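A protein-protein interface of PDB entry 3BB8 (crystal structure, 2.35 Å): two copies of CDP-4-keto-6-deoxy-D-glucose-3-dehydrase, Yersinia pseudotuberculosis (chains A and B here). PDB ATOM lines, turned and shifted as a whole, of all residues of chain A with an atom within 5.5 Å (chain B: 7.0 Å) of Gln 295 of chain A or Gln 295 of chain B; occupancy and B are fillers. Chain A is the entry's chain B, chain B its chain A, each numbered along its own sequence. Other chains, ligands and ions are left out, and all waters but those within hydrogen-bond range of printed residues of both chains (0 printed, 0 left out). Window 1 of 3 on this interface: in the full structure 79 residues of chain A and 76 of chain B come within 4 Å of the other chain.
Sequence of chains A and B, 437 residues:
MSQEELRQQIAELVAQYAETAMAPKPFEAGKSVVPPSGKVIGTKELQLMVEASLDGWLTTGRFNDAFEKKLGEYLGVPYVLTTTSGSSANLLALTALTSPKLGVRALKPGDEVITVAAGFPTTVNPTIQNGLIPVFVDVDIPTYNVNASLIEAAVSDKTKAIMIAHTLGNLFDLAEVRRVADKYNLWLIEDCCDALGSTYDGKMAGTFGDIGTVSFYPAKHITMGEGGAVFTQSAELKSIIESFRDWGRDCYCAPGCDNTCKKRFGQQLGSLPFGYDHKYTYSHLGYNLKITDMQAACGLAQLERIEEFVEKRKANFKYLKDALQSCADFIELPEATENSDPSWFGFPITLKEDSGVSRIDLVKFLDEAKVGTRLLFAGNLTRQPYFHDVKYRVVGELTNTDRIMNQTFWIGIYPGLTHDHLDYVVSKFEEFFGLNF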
ATOM      1  N   THR A  84       9.028 -18.445   0.812  1.00  0.00           N
ATOM      2  CA  THR A  84      10.259 -18.610   1.591  1.00  0.00           C
ATOM      3  C   THR A  84      10.221 -19.333   2.932  1.00  0.00           C
ATOM      4  O   THR A  84      11.249 -19.853   3.379  1.00  0.00           O
ATOM      5  CB  THR A  84      10.977 -17.245   1.835  1.00  0.00           C
ATOM      6  OG1 THR A  84      10.429 -16.605   3.002  1.00  0.00           O
ATOM      7  CG2 THR A  84      10.815 -16.337   0.612  1.00  0.00           C
ATOM      8  N   THR A 223      11.302 -30.940   4.606  1.00  0.00           N
ATOM      9  CA  THR A 223      12.049 -29.700   4.495  1.00  0.00           C
ATOM     10  C   THR A 223      12.652 -29.324   3.128  1.00  0.00           C
ATOM     11  O   THR A 223      12.745 -30.142   2.215  1.00  0.00           O
ATOM     12  CB  THR A 223      13.175 -29.702   5.540  1.00  0.00           C
ATOM     13  OG1 THR A 223      13.855 -28.436   5.528  1.00  0.00           O
ATOM     14  CG2 THR A 223      14.166 -30.818   5.229  1.00  0.00           C
ATOM     15  N   MET A 224      13.049 -28.057   3.025  1.00  0.00           N
ATOM     16  CA  MET A 224      13.683 -27.476   1.842  1.00  0.00           C
ATOM     17  C   MET A 224      14.824 -26.648   2.408  1.00  0.00           C
ATOM     18  O   MET A 224      15.477 -25.893   1.678  1.00  0.00           O
ATOM     19  CB  MET A 224      12.761 -26.492   1.117  1.00  0.00           C
ATOM     20  CG  MET A 224      11.515 -27.039   0.474  1.00  0.00           C
ATOM     21  SD  MET A 224      10.788 -25.685  -0.501  1.00  0.00           S
ATOM     22  CE  MET A 224       9.267 -26.449  -1.128  1.00  0.00           C
ATOM     23  N   GLU A 226      14.821 -23.980   3.998  1.00  0.00           N
ATOM     24  CA  GLU A 226      13.979 -22.828   4.292  1.00  0.00           C
ATOM     25  C   GLU A 226      12.934 -22.892   3.188  1.00  0.00           C
ATOM     26  O   GLU A 226      13.289 -23.022   2.018  1.00  0.00           O
ATOM     27  CB  GLU A 226      14.754 -21.507   4.169  1.00  0.00           C
ATOM     28  CG  GLU A 226      15.744 -21.221   5.282  1.00  0.00           C
ATOM     29  CD  GLU A 226      15.078 -21.191   6.639  1.00  0.00           C
ATOM     30  OE1 GLU A 226      13.883 -20.840   6.692  1.00  0.00           O
ATOM     31  OE2 GLU A 226      15.739 -21.510   7.649  1.00  0.00           O
ATOM     32  N   GLY A 227      11.658 -22.821   3.552  1.00  0.00           N
ATOM     33  CA  GLY A 227      10.620 -22.864   2.546  1.00  0.00           C
ATOM     34  C   GLY A 227       9.259 -22.959   3.189  1.00  0.00           C
ATOM     35  O   GLY A 227       9.149 -23.234   4.383  1.00  0.00           O
ATOM     36  N   ILE A 291      11.001 -18.642  -3.887  1.00  0.00           N
ATOM     37  CA  ILE A 291      12.124 -19.512  -3.578  1.00  0.00           C
ATOM     38  C   ILE A 291      12.855 -19.917  -4.852  1.00  0.00           C
ATOM     39  O   ILE A 291      12.512 -19.457  -5.945  1.00  0.00           O
ATOM     40  CB  ILE A 291      11.659 -20.788  -2.867  1.00  0.00           C
ATOM     41  CG1 ILE A 291      10.710 -21.577  -3.774  1.00  0.00           C
ATOM     42  CG2 ILE A 291      10.957 -20.422  -1.574  1.00  0.00           C
ATOM     43  CD1 ILE A 291      10.449 -22.998  -3.294  1.00  0.00           C
ATOM     44  N   THR A 292      13.863 -20.768  -4.695  1.00  0.00           N
ATOM     45  CA  THR A 292      14.655 -21.256  -5.815  1.00  0.00           C
ATOM     46  C   THR A 292      14.237 -22.695  -6.135  1.00  0.00           C
ATOM     47  O   THR A 292      13.609 -23.367  -5.310  1.00  0.00           O
ATOM     48  CB  THR A 292      16.167 -21.258  -5.483  1.00  0.00           C
ATOM     49  OG1 THR A 292      16.433 -22.248  -4.482  1.00  0.00           O
ATOM     50  CG2 THR A 292      16.613 -19.894  -4.982  1.00  0.00           C
ATOM     51  N   ASP A 293      14.592 -23.171  -7.324  1.00  0.00           N
ATOM     52  CA  ASP A 293      14.232 -24.526  -7.721  1.00  0.00           C
ATOM     53  C   ASP A 293      15.096 -25.555  -6.973  1.00  0.00           C
ATOM     54  O   ASP A 293      14.777 -26.745  -6.950  1.00  0.00           O
ATOM     55  CB  ASP A 293      14.370 -24.680  -9.246  1.00  0.00           C
ATOM     56  CG  ASP A 293      13.204 -25.458  -9.871  1.00  0.00           C
ATOM     57  OD1 ASP A 293      12.035 -25.225  -9.484  1.00  0.00           O
ATOM     58  OD2 ASP A 293      13.458 -26.294 -10.763  1.00  0.00           O
ATOM     59  N   MET A 294      16.189 -25.096  -6.363  1.00  0.00           N
ATOM     60  CA  MET A 294      17.040 -25.992  -5.580  1.00  0.00           C
ATOM     61  C   MET A 294      16.227 -26.414  -4.349  1.00  0.00           C
ATOM     62  O   MET A 294      16.170 -27.589  -3.982  1.00  0.00           O
ATOM     63  CB  MET A 294      18.319 -25.283  -5.119  1.00  0.00           C
ATOM     64  CG  MET A 294      19.313 -24.964  -6.220  1.00  0.00           C
ATOM     65  SD  MET A 294      18.945 -23.458  -7.151  1.00  0.00           S
ATOM     66  CE  MET A 294      19.756 -22.223  -6.132  1.00  0.00           C
ATOM     67  N   GLN A 295      15.589 -25.435  -3.722  1.00  0.00           N
ATOM     68  CA  GLN A 295      14.769 -25.686  -2.546  1.00  0.00           C
ATOM     69  C   GLN A 295      13.583 -26.541  -2.956  1.00  0.00           C
ATOM     70  O   GLN A 295      13.177 -27.445  -2.221  1.00  0.00           O
ATOM     71  CB  GLN A 295      14.270 -24.361  -1.957  1.00  0.00           C
ATOM     72  CG  GLN A 295      15.359 -23.504  -1.341  1.00  0.00           C
ATOM     73  CD  GLN A 295      14.975 -22.031  -1.259  1.00  0.00           C
ATOM     74  OE1 GLN A 295      15.141 -21.274  -2.228  1.00  0.00           O
ATOM     75  NE2 GLN A 295      14.451 -21.618  -0.109  1.00  0.00           N
ATOM     76  N   ALA A 296      13.024 -26.244  -4.127  1.00  0.00           N
ATOM     77  CA  ALA A 296      11.875 -26.988  -4.629  1.00  0.00           C
ATOM     78  C   ALA A 296      12.215 -28.472  -4.782  1.00  0.00           C
ATOM     79  O   ALA A 296      11.437 -29.339  -4.383  1.00  0.00           O
ATOM     80  CB  ALA A 296      11.432 -26.416  -5.967  1.00  0.00           C
ATOM     81  N   ALA A 297      13.382 -28.753  -5.356  1.00  0.00           N
ATOM     82  CA  ALA A 297      13.823 -30.130  -5.572  1.00  0.00           C
ATOM     83  C   ALA A 297      13.805 -30.895  -4.260  1.00  0.00           C
ATOM     84  O   ALA A 297      13.161 -31.948  -4.149  1.00  0.00           O
ATOM     85  CB  ALA A 297      15.232 -30.149  -6.169  1.00  0.00           C
ATOM     86  N   CYS A 298      14.507 -30.363  -3.265  1.00  0.00           N
ATOM     87  CA  CYS A 298      14.560 -31.008  -1.963  1.00  0.00           C
ATOM     88  C   CYS A 298      13.138 -31.320  -1.519  1.00  0.00           C
ATOM     89  O   CYS A 298      12.824 -32.453  -1.156  1.00  0.00           O
ATOM     90  CB  CYS A 298      15.249 -30.092  -0.957  1.00  0.00           C
ATOM     91  SG  CYS A 298      15.724 -30.891   0.588  1.00  0.00           S
ATOM     92  N   GLY A 299      12.265 -30.320  -1.583  1.00  0.00           N
ATOM     93  CA  GLY A 299      10.886 -30.530  -1.189  1.00  0.00           C
ATOM     94  C   GLY A 299      10.227 -31.664  -1.957  1.00  0.00           C
ATOM     95  O   GLY A 299       9.468 -32.454  -1.383  1.00  0.00           O
ATOM     96  N   LEU A 300      10.517 -31.747  -3.257  1.00  0.00           N
ATOM     97  CA  LEU A 300       9.937 -32.782  -4.119  1.00  0.00           C
ATOM     98  C   LEU A 300      10.323 -34.192  -3.685  1.00  0.00           C
ATOM     99  O   LEU A 300       9.484 -35.090  -3.670  1.00  0.00           O
ATOM    100  CB  LEU A 300      10.349 -32.553  -5.580  1.00  0.00           C
ATOM    101  CG  LEU A 300       9.703 -33.487  -6.614  1.00  0.00           C
ATOM    102  CD1 LEU A 300       8.177 -33.436  -6.499  1.00  0.00           C
ATOM    103  CD2 LEU A 300      10.156 -33.079  -8.010  1.00  0.00           C
ATOM    104  N   MET B  49      27.026 -25.316  -5.599  1.00  0.00           N
ATOM    105  CA  MET B  49      25.653 -25.692  -5.285  1.00  0.00           C
ATOM    106  C   MET B  49      25.568 -27.191  -5.022  1.00  0.00           C
ATOM    107  O   MET B  49      24.753 -27.645  -4.216  1.00  0.00           O
ATOM    108  CB  MET B  49      24.702 -25.300  -6.416  1.00  0.00           C
ATOM    109  CG  MET B  49      24.492 -23.805  -6.523  1.00  0.00           C
ATOM    110  SD  MET B  49      23.087 -23.415  -7.559  1.00  0.00           S
ATOM    111  CE  MET B  49      23.805 -23.693  -9.196  1.00  0.00           C
ATOM    112  N   ALA B  52      27.031 -27.784  -1.453  1.00  0.00           N
ATOM    113  CA  ALA B  52      26.014 -27.446  -0.468  1.00  0.00           C
ATOM    114  C   ALA B  52      24.926 -28.517  -0.448  1.00  0.00           C
ATOM    115  O   ALA B  52      24.450 -28.909   0.613  1.00  0.00           O
ATOM    116  CB  ALA B  52      25.413 -26.085  -0.790  1.00  0.00           C
ATOM    117  N   LEU B  58      21.380 -27.749   4.445  1.00  0.00           N
ATOM    118  CA  LEU B  58      20.237 -27.002   3.912  1.00  0.00           C
ATOM    119  C   LEU B  58      20.063 -25.550   4.378  1.00  0.00           C
ATOM    120  O   LEU B  58      20.021 -24.638   3.545  1.00  0.00           O
ATOM    121  CB  LEU B  58      18.947 -27.783   4.183  1.00  0.00           C
ATOM    122  CG  LEU B  58      19.000 -29.277   3.831  1.00  0.00           C
ATOM    123  CD1 LEU B  58      17.610 -29.871   3.910  1.00  0.00           C
ATOM    124  CD2 LEU B  58      19.561 -29.468   2.436  1.00  0.00           C
ATOM    125  N   PHE B  63      28.614 -22.098   3.589  1.00  0.00           N
ATOM    126  CA  PHE B  63      28.623 -21.169   2.465  1.00  0.00           C
ATOM    127  C   PHE B  63      28.066 -19.782   2.775  1.00  0.00           C
ATOM    128  O   PHE B  63      28.641 -18.772   2.343  1.00  0.00           O
ATOM    129  CB  PHE B  63      27.877 -21.764   1.278  1.00  0.00           C
ATOM    130  CG  PHE B  63      28.543 -22.968   0.699  1.00  0.00           C
ATOM    131  CD1 PHE B  63      28.116 -24.249   1.040  1.00  0.00           C
ATOM    132  CD2 PHE B  63      29.611 -22.825  -0.183  1.00  0.00           C
ATOM    133  CE1 PHE B  63      28.740 -25.367   0.509  1.00  0.00           C
ATOM    134  CE2 PHE B  63      30.243 -23.933  -0.718  1.00  0.00           C
ATOM    135  CZ  PHE B  63      29.809 -25.209  -0.374  1.00  0.00           C
ATOM    136  N   ASN B  64      26.962 -19.719   3.520  1.00  0.00           N
ATOM    137  CA  ASN B  64      26.381 -18.426   3.846  1.00  0.00           C
ATOM    138  C   ASN B  64      27.366 -17.583   4.636  1.00  0.00           C
ATOM    139  O   ASN B  64      27.407 -16.362   4.473  1.00  0.00           O
ATOM    140  CB  ASN B  64      25.086 -18.577   4.646  1.00  0.00           C
ATOM    141  CG  ASN B  64      24.376 -17.241   4.859  1.00  0.00           C
ATOM    142  OD1 ASN B  64      23.861 -16.645   3.910  1.00  0.00           O
ATOM    143  ND2 ASN B  64      24.362 -16.760   6.104  1.00  0.00           N
ATOM    144  N   PHE B  67      29.950 -16.329   2.144  1.00  0.00           N
ATOM    145  CA  PHE B  67      29.363 -15.297   1.301  1.00  0.00           C
ATOM    146  C   PHE B  67      29.234 -13.963   2.012  1.00  0.00           C
ATOM    147  O   PHE B  67      29.664 -12.938   1.488  1.00  0.00           O
ATOM    148  CB  PHE B  67      27.982 -15.726   0.778  1.00  0.00           C
ATOM    149  CG  PHE B  67      27.321 -14.683  -0.089  1.00  0.00           C
ATOM    150  CD1 PHE B  67      26.525 -13.687   0.477  1.00  0.00           C
ATOM    151  CD2 PHE B  67      27.578 -14.635  -1.459  1.00  0.00           C
ATOM    152  CE1 PHE B  67      25.999 -12.655  -0.302  1.00  0.00           C
ATOM    153  CE2 PHE B  67      27.056 -13.604  -2.247  1.00  0.00           C
ATOM    154  CZ  PHE B  67      26.267 -12.612  -1.665  1.00  0.00           C
ATOM    155  N   THR B  83      19.236 -12.452   2.893  1.00  0.00           N
ATOM    156  CA  THR B  83      17.789 -12.567   3.020  1.00  0.00           C
ATOM    157  C   THR B  83      17.202 -13.128   1.716  1.00  0.00           C
ATOM    158  O   THR B  83      17.943 -13.364   0.766  1.00  0.00           O
ATOM    159  CB  THR B  83      17.169 -11.205   3.402  1.00  0.00           C
ATOM    160  OG1 THR B  83      15.761 -11.361   3.592  1.00  0.00           O
ATOM    161  CG2 THR B  83      17.450 -10.166   2.342  1.00  0.00           C
ATOM    162  N   THR B  84      15.887 -13.342   1.662  1.00  0.00           N
ATOM    163  CA  THR B  84      15.260 -13.970   0.492  1.00  0.00           C
ATOM    164  C   THR B  84      15.308 -13.256  -0.858  1.00  0.00           C
ATOM    165  O   THR B  84      15.239 -13.904  -1.897  1.00  0.00           O
ATOM    166  CB  THR B  84      13.779 -14.282   0.750  1.00  0.00           C
ATOM    167  OG1 THR B  84      12.999 -13.121   0.441  1.00  0.00           O
ATOM    168  CG2 THR B  84      13.554 -14.679   2.221  1.00  0.00           C
ATOM    169  N   SER B  85      15.419 -11.934  -0.851  1.00  0.00           N
ATOM    170  CA  SER B  85      15.418 -11.186  -2.090  1.00  0.00           C
ATOM    171  C   SER B  85      15.793  -9.745  -1.819  1.00  0.00           C
ATOM    172  O   SER B  85      15.906  -9.328  -0.668  1.00  0.00           O
ATOM    173  CB  SER B  85      14.002 -11.208  -2.694  1.00  0.00           C
ATOM    174  OG  SER B  85      13.070 -10.569  -1.823  1.00  0.00           O
ATOM    175  N   PHE B 216      19.820 -10.430  -5.510  1.00  0.00           N
ATOM    176  CA  PHE B 216      20.516 -11.468  -6.269  1.00  0.00           C
ATOM    177  C   PHE B 216      19.581 -12.219  -7.208  1.00  0.00           C
ATOM    178  O   PHE B 216      19.736 -13.424  -7.435  1.00  0.00           O
ATOM    179  CB  PHE B 216      21.216 -12.454  -5.331  1.00  0.00           C
ATOM    180  CG  PHE B 216      22.115 -11.797  -4.342  1.00  0.00           C
ATOM    181  CD1 PHE B 216      22.056 -12.145  -2.992  1.00  0.00           C
ATOM    182  CD2 PHE B 216      23.001 -10.806  -4.741  1.00  0.00           C
ATOM    183  CE1 PHE B 216      22.872 -11.507  -2.053  1.00  0.00           C
ATOM    184  CE2 PHE B 216      23.821 -10.161  -3.806  1.00  0.00           C
ATOM    185  CZ  PHE B 216      23.753 -10.515  -2.461  1.00  0.00           C
ATOM    186  N   THR B 223      23.934 -13.531  -9.000  1.00  0.00           N
ATOM    187  CA  THR B 223      22.684 -14.175  -8.621  1.00  0.00           C
ATOM    188  C   THR B 223      22.733 -15.414  -7.713  1.00  0.00           C
ATOM    189  O   THR B 223      23.753 -16.103  -7.609  1.00  0.00           O
ATOM    190  CB  THR B 223      21.912 -14.561  -9.888  1.00  0.00           C
ATOM    191  OG1 THR B 223      20.618 -15.074  -9.541  1.00  0.00           O
ATOM    192  CG2 THR B 223      22.685 -15.629 -10.647  1.00  0.00           C
ATOM    193  N   MET B 224      21.611 -15.689  -7.055  1.00  0.00           N
ATOM    194  CA  MET B 224      21.428 -16.951  -6.348  1.00  0.00           C
ATOM    195  C   MET B 224      20.144 -17.663  -6.758  1.00  0.00           C
ATOM    196  O   MET B 224      19.612 -18.484  -6.011  1.00  0.00           O
ATOM    197  CB  MET B 224      21.241 -16.703  -4.849  1.00  0.00           C
ATOM    198  CG  MET B 224      22.442 -16.063  -4.171  1.00  0.00           C
ATOM    199  SD  MET B 224      22.249 -15.944  -2.383  1.00  0.00           S
ATOM    200  CE  MET B 224      23.473 -14.696  -1.992  1.00  0.00           C
ATOM    201  N   GLY B 225      19.650 -17.342  -7.949  1.00  0.00           N
ATOM    202  CA  GLY B 225      18.229 -17.419  -8.231  1.00  0.00           C
ATOM    203  C   GLY B 225      17.343 -16.384  -7.566  1.00  0.00           C
ATOM    204  O   GLY B 225      16.847 -15.466  -8.218  1.00  0.00           O
ATOM    205  N   GLU B 226      17.144 -16.534  -6.260  1.00  0.00           N
ATOM    206  CA  GLU B 226      16.352 -15.584  -5.493  1.00  0.00           C
ATOM    207  C   GLU B 226      17.203 -15.377  -4.246  1.00  0.00           C
ATOM    208  O   GLU B 226      17.710 -16.347  -3.678  1.00  0.00           O
ATOM    209  CB  GLU B 226      14.988 -16.157  -5.108  1.00  0.00           C
ATOM    210  CG  GLU B 226      14.052 -16.411  -6.280  1.00  0.00           C
ATOM    211  CD  GLU B 226      13.319 -15.165  -6.772  1.00  0.00           C
ATOM    212  OE1 GLU B 226      13.596 -14.042  -6.288  1.00  0.00           O
ATOM    213  OE2 GLU B 226      12.454 -15.322  -7.658  1.00  0.00           O
ATOM    214  N   GLY B 227      17.396 -14.120  -3.861  1.00  0.00           N
ATOM    215  CA  GLY B 227      18.182 -13.820  -2.685  1.00  0.00           C
ATOM    216  C   GLY B 227      18.580 -12.362  -2.674  1.00  0.00           C
ATOM    217  O   GLY B 227      18.461 -11.674  -3.691  1.00  0.00           O
ATOM    218  N   GLY B 228      19.046 -11.885  -1.525  1.00  0.00           N
ATOM    219  CA  GLY B 228      19.481 -10.508  -1.403  1.00  0.00           C
ATOM    220  C   GLY B 228      20.245 -10.356  -0.101  1.00  0.00           C
ATOM    221  O   GLY B 228      20.491 -11.355   0.578  1.00  0.00           O
ATOM    222  N   LYS B 290      14.931 -15.866   5.717  1.00  0.00           N
ATOM    223  CA  LYS B 290      16.284 -16.405   5.529  1.00  0.00           C
ATOM    224  C   LYS B 290      16.342 -17.280   4.278  1.00  0.00           C
ATOM    225  O   LYS B 290      15.305 -17.694   3.745  1.00  0.00           O
ATOM    226  CB  LYS B 290      16.730 -17.245   6.735  1.00  0.00           C
ATOM    227  CG  LYS B 290      16.714 -16.508   8.060  1.00  0.00           C
ATOM    228  CD  LYS B 290      17.366 -17.323   9.176  1.00  0.00           C
ATOM    229  CE  LYS B 290      16.364 -17.726  10.261  1.00  0.00           C
ATOM    230  NZ  LYS B 290      15.295 -18.658   9.782  1.00  0.00           N
ATOM    231  N   ILE B 291      17.555 -17.557   3.810  1.00  0.00           N
ATOM    232  CA  ILE B 291      17.719 -18.395   2.632  1.00  0.00           C
ATOM    233  C   ILE B 291      18.441 -19.687   2.979  1.00  0.00           C
ATOM    234  O   ILE B 291      18.704 -19.971   4.154  1.00  0.00           O
ATOM    235  CB  ILE B 291      18.475 -17.666   1.476  1.00  0.00           C
ATOM    236  CG1 ILE B 291      19.989 -17.621   1.734  1.00  0.00           C
ATOM    237  CG2 ILE B 291      17.909 -16.266   1.306  1.00  0.00           C
ATOM    238  CD1 ILE B 291      20.414 -16.688   2.820  1.00  0.00           C
ATOM    239  N   THR B 292      18.731 -20.478   1.954  1.00  0.00           N
ATOM    240  CA  THR B 292      19.405 -21.756   2.133  1.00  0.00           C
ATOM    241  C   THR B 292      20.891 -21.628   1.812  1.00  0.00           C
ATOM    242  O   THR B 292      21.315 -20.653   1.188  1.00  0.00           O
ATOM    243  CB  THR B 292      18.804 -22.824   1.200  1.00  0.00           C
ATOM    244  OG1 THR B 292      19.121 -22.499  -0.159  1.00  0.00           O
ATOM    245  CG2 THR B 292      17.295 -22.890   1.369  1.00  0.00           C
ATOM    246  N   ASP B 293      21.687 -22.611   2.226  1.00  0.00           N
ATOM    247  CA  ASP B 293      23.113 -22.541   1.944  1.00  0.00           C
ATOM    248  C   ASP B 293      23.302 -22.806   0.449  1.00  0.00           C
ATOM    249  O   ASP B 293      24.302 -22.388  -0.135  1.00  0.00           O
ATOM    250  CB  ASP B 293      23.892 -23.552   2.803  1.00  0.00           C
ATOM    251  CG  ASP B 293      25.217 -22.983   3.330  1.00  0.00           C
ATOM    252  OD1 ASP B 293      25.244 -21.812   3.763  1.00  0.00           O
ATOM    253  OD2 ASP B 293      26.233 -23.713   3.326  1.00  0.00           O
ATOM    254  N   MET B 294      22.329 -23.482  -0.169  1.00  0.00           N
ATOM    255  CA  MET B 294      22.391 -23.756  -1.604  1.00  0.00           C
ATOM    256  C   MET B 294      22.499 -22.424  -2.340  1.00  0.00           C
ATOM    257  O   MET B 294      23.387 -22.220  -3.176  1.00  0.00           O
ATOM    258  CB  MET B 294      21.139 -24.485  -2.083  1.00  0.00           C
ATOM    259  CG  MET B 294      21.025 -25.912  -1.608  1.00  0.00           C
ATOM    260  SD  MET B 294      20.435 -26.118   0.097  1.00  0.00           S
ATOM    261  CE  MET B 294      18.666 -25.964  -0.147  1.00  0.00           C
ATOM    262  N   GLN B 295      21.581 -21.519  -2.019  1.00  0.00           N
ATOM    263  CA  GLN B 295      21.583 -20.194  -2.611  1.00  0.00           C
ATOM    264  C   GLN B 295      22.895 -19.512  -2.244  1.00  0.00           C
ATOM    265  O   GLN B 295      23.547 -18.898  -3.088  1.00  0.00           O
ATOM    266  CB  GLN B 295      20.399 -19.372  -2.078  1.00  0.00           C
ATOM    267  CG  GLN B 295      19.039 -19.814  -2.600  1.00  0.00           C
ATOM    268  CD  GLN B 295      17.891 -19.474  -1.648  1.00  0.00           C
ATOM    269  OE1 GLN B 295      17.569 -20.242  -0.737  1.00  0.00           O
ATOM    270  NE2 GLN B 295      17.279 -18.317  -1.851  1.00  0.00           N
ATOM    271  N   ALA B 296      23.282 -19.614  -0.979  1.00  0.00           N
ATOM    272  CA  ALA B 296      24.528 -19.001  -0.526  1.00  0.00           C
ATOM    273  C   ALA B 296      25.715 -19.445  -1.392  1.00  0.00           C
ATOM    274  O   ALA B 296      26.582 -18.640  -1.727  1.00  0.00           O
ATOM    275  CB  ALA B 296      24.792 -19.362   0.936  1.00  0.00           C
ATOM    276  N   ALA B 297      25.741 -20.725  -1.747  1.00  0.00           N
ATOM    277  CA  ALA B 297      26.817 -21.287  -2.559  1.00  0.00           C
ATOM    278  C   ALA B 297      26.913 -20.591  -3.912  1.00  0.00           C
ATOM    279  O   ALA B 297      27.979 -20.088  -4.291  1.00  0.00           O
ATOM    280  CB  ALA B 297      26.586 -22.788  -2.764  1.00  0.00           C
ATOM    281  N   CYS B 298      25.793 -20.571  -4.634  1.00  0.00           N
ATOM    282  CA  CYS B 298      25.737 -19.944  -5.945  1.00  0.00           C
ATOM    283  C   CYS B 298      26.279 -18.532  -5.828  1.00  0.00           C
ATOM    284  O   CYS B 298      27.119 -18.116  -6.615  1.00  0.00           O
ATOM    285  CB  CYS B 298      24.296 -19.923  -6.457  1.00  0.00           C
ATOM    286  SG  CYS B 298      24.104 -19.464  -8.201  1.00  0.00           S
ATOM    287  N   GLY B 299      25.812 -17.805  -4.824  1.00  0.00           N
ATOM    288  CA  GLY B 299      26.276 -16.447  -4.627  1.00  0.00           C
ATOM    289  C   GLY B 299      27.768 -16.354  -4.375  1.00  0.00           C
ATOM    290  O   GLY B 299      28.427 -15.440  -4.864  1.00  0.00           O
ATOM    291  N   LEU B 300      28.315 -17.300  -3.611  1.00  0.00           N
ATOM    292  CA  LEU B 300      29.749 -17.283  -3.303  1.00  0.00           C
ATOM    293  C   LEU B 300      30.578 -17.398  -4.579  1.00  0.00           C
ATOM    294  O   LEU B 300      31.501 -16.616  -4.789  1.00  0.00           O
ATOM    295  CB  LEU B 300      30.114 -18.409  -2.331  1.00  0.00           C
ATOM    296  CG  LEU B 300      31.565 -18.402  -1.835  1.00  0.00           C
ATOM    297  CD1 LEU B 300      31.891 -17.085  -1.145  1.00  0.00           C
ATOM    298  CD2 LEU B 300      31.766 -19.562  -0.887  1.00  0.00           C
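OE1 of Gln 295 of chain B lies close to OE1 of Gln 295 of chain A. NZ of Lys 290 of chain B is in salt-bridge range of OE2 of Glu 226 of chain A (3.6 Å).
OG1 of Thr 292 of chain B sits at hydrogen-bond distance from OE1 of Gln 295 of chain B, 2.8 Å away. OG1 of Thr 292 of chain A sits close to N of Met 294 of chain A (3.4 Å). The side-chain hydroxyl (OG) of Ser 85 of chain B sits at hydrogen-bond distance from the side-chain hydroxyl (OG1) of Thr 84 of chain B (3.4 Å). The side-chain amide nitrogen (NE2) of Gln 295 of chain A is in hydrogen-bond range of the backbone carbonyl oxygen (O) of Glu 226 of chain A (2.8 Å).
Thr 84 of chain B touches Thr 84 of chain A (CG2 to CG2, 3.6 Å). Leu 58 of chain B touches Thr 223 of chain A (CD1 to CG2, 3.8 Å). Thr 292 of chain B touches Met 224 of chain A. CE of Met 294 of chain B touches O of Met 224 of chain A (3.7 Å). Glu 226 of chain A touches Ile 291 of chain B (CG to O, 3.4 Å). Thr 292 of chain B touches Glu 226 of chain A. Thr 292 of chain A touches Met 224 of chain B. CG2 of Thr 292 of chain A touches N of Glu 226 of chain B, 3.6 Å away. CE of Met 294 of chain A touches SD of Met 49 of chain B (3.8 Å). Thr 292 of chain B touches Gln 295 of chain A (CG2 to CG, 3.4 Å).
Printed residues of chain B within 4 Å of Ile 291 of chain A: Glu 226. Of the printed residues of chain B, Met 294 of chain A touches Met 49 and Met 224. Gln 295 of chain A touches just these residues of chain B: Thr 292 and Gln 295. Printed residues of chain A within 4 Å of Leu 58 of chain B: Thr 223 and Cys 298. Gly 225 of chain B touches none of the printed residues of chain A. Asp 293 of chain B touches none of the printed residues of chain A. Of chain A, only Thr 292 and Gln 295 come within 4 Å of Gln 295 of chain B. The nearest residue of chain B that does not touch Gln 295 of chain A is Met 294 of chain B (4.3 Å).
Hydrophobic or aromatic side chains of chain A within 4 Å of the printed part of chain B: Met 294. Of the 27 printed residues of chain B, 10 touch a printed residue of chain A. Printed residues of chain B that touch a printed residue of chain A: Met 49, Leu 58, Thr 84, Met 224, Glu 226, Lys 290, Ile 291, Thr 292, Met 294 and Gln 295. Among the printed residues, 16 pairs touch across the chains. Among the printed residues, Asp or Glu carboxylates within 4 Å of a Lys or Arg side-chain nitrogen of the other chain: Glu 226 of chain A with Lys 290 of chain B.
Met 224 of chain A touches Met 294 of chain B, and with the chains exchanged Met 294 of chain A touches Met 224 of chain B. Glu 226 of chain A touches Ile 291 of chain B, and with the chains exchanged Ile 291 of chain A touches Glu 226 of chain B. Glu 226 of chain A touches Thr 292 of chain B, and with the chains exchanged Thr 292 of chain A touches Glu 226 of chain B. Thr 292 of chain A touches Gln 295 of chain B, and with the chains exchanged Gln 295 of chain A touches Thr 292 of chain B.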
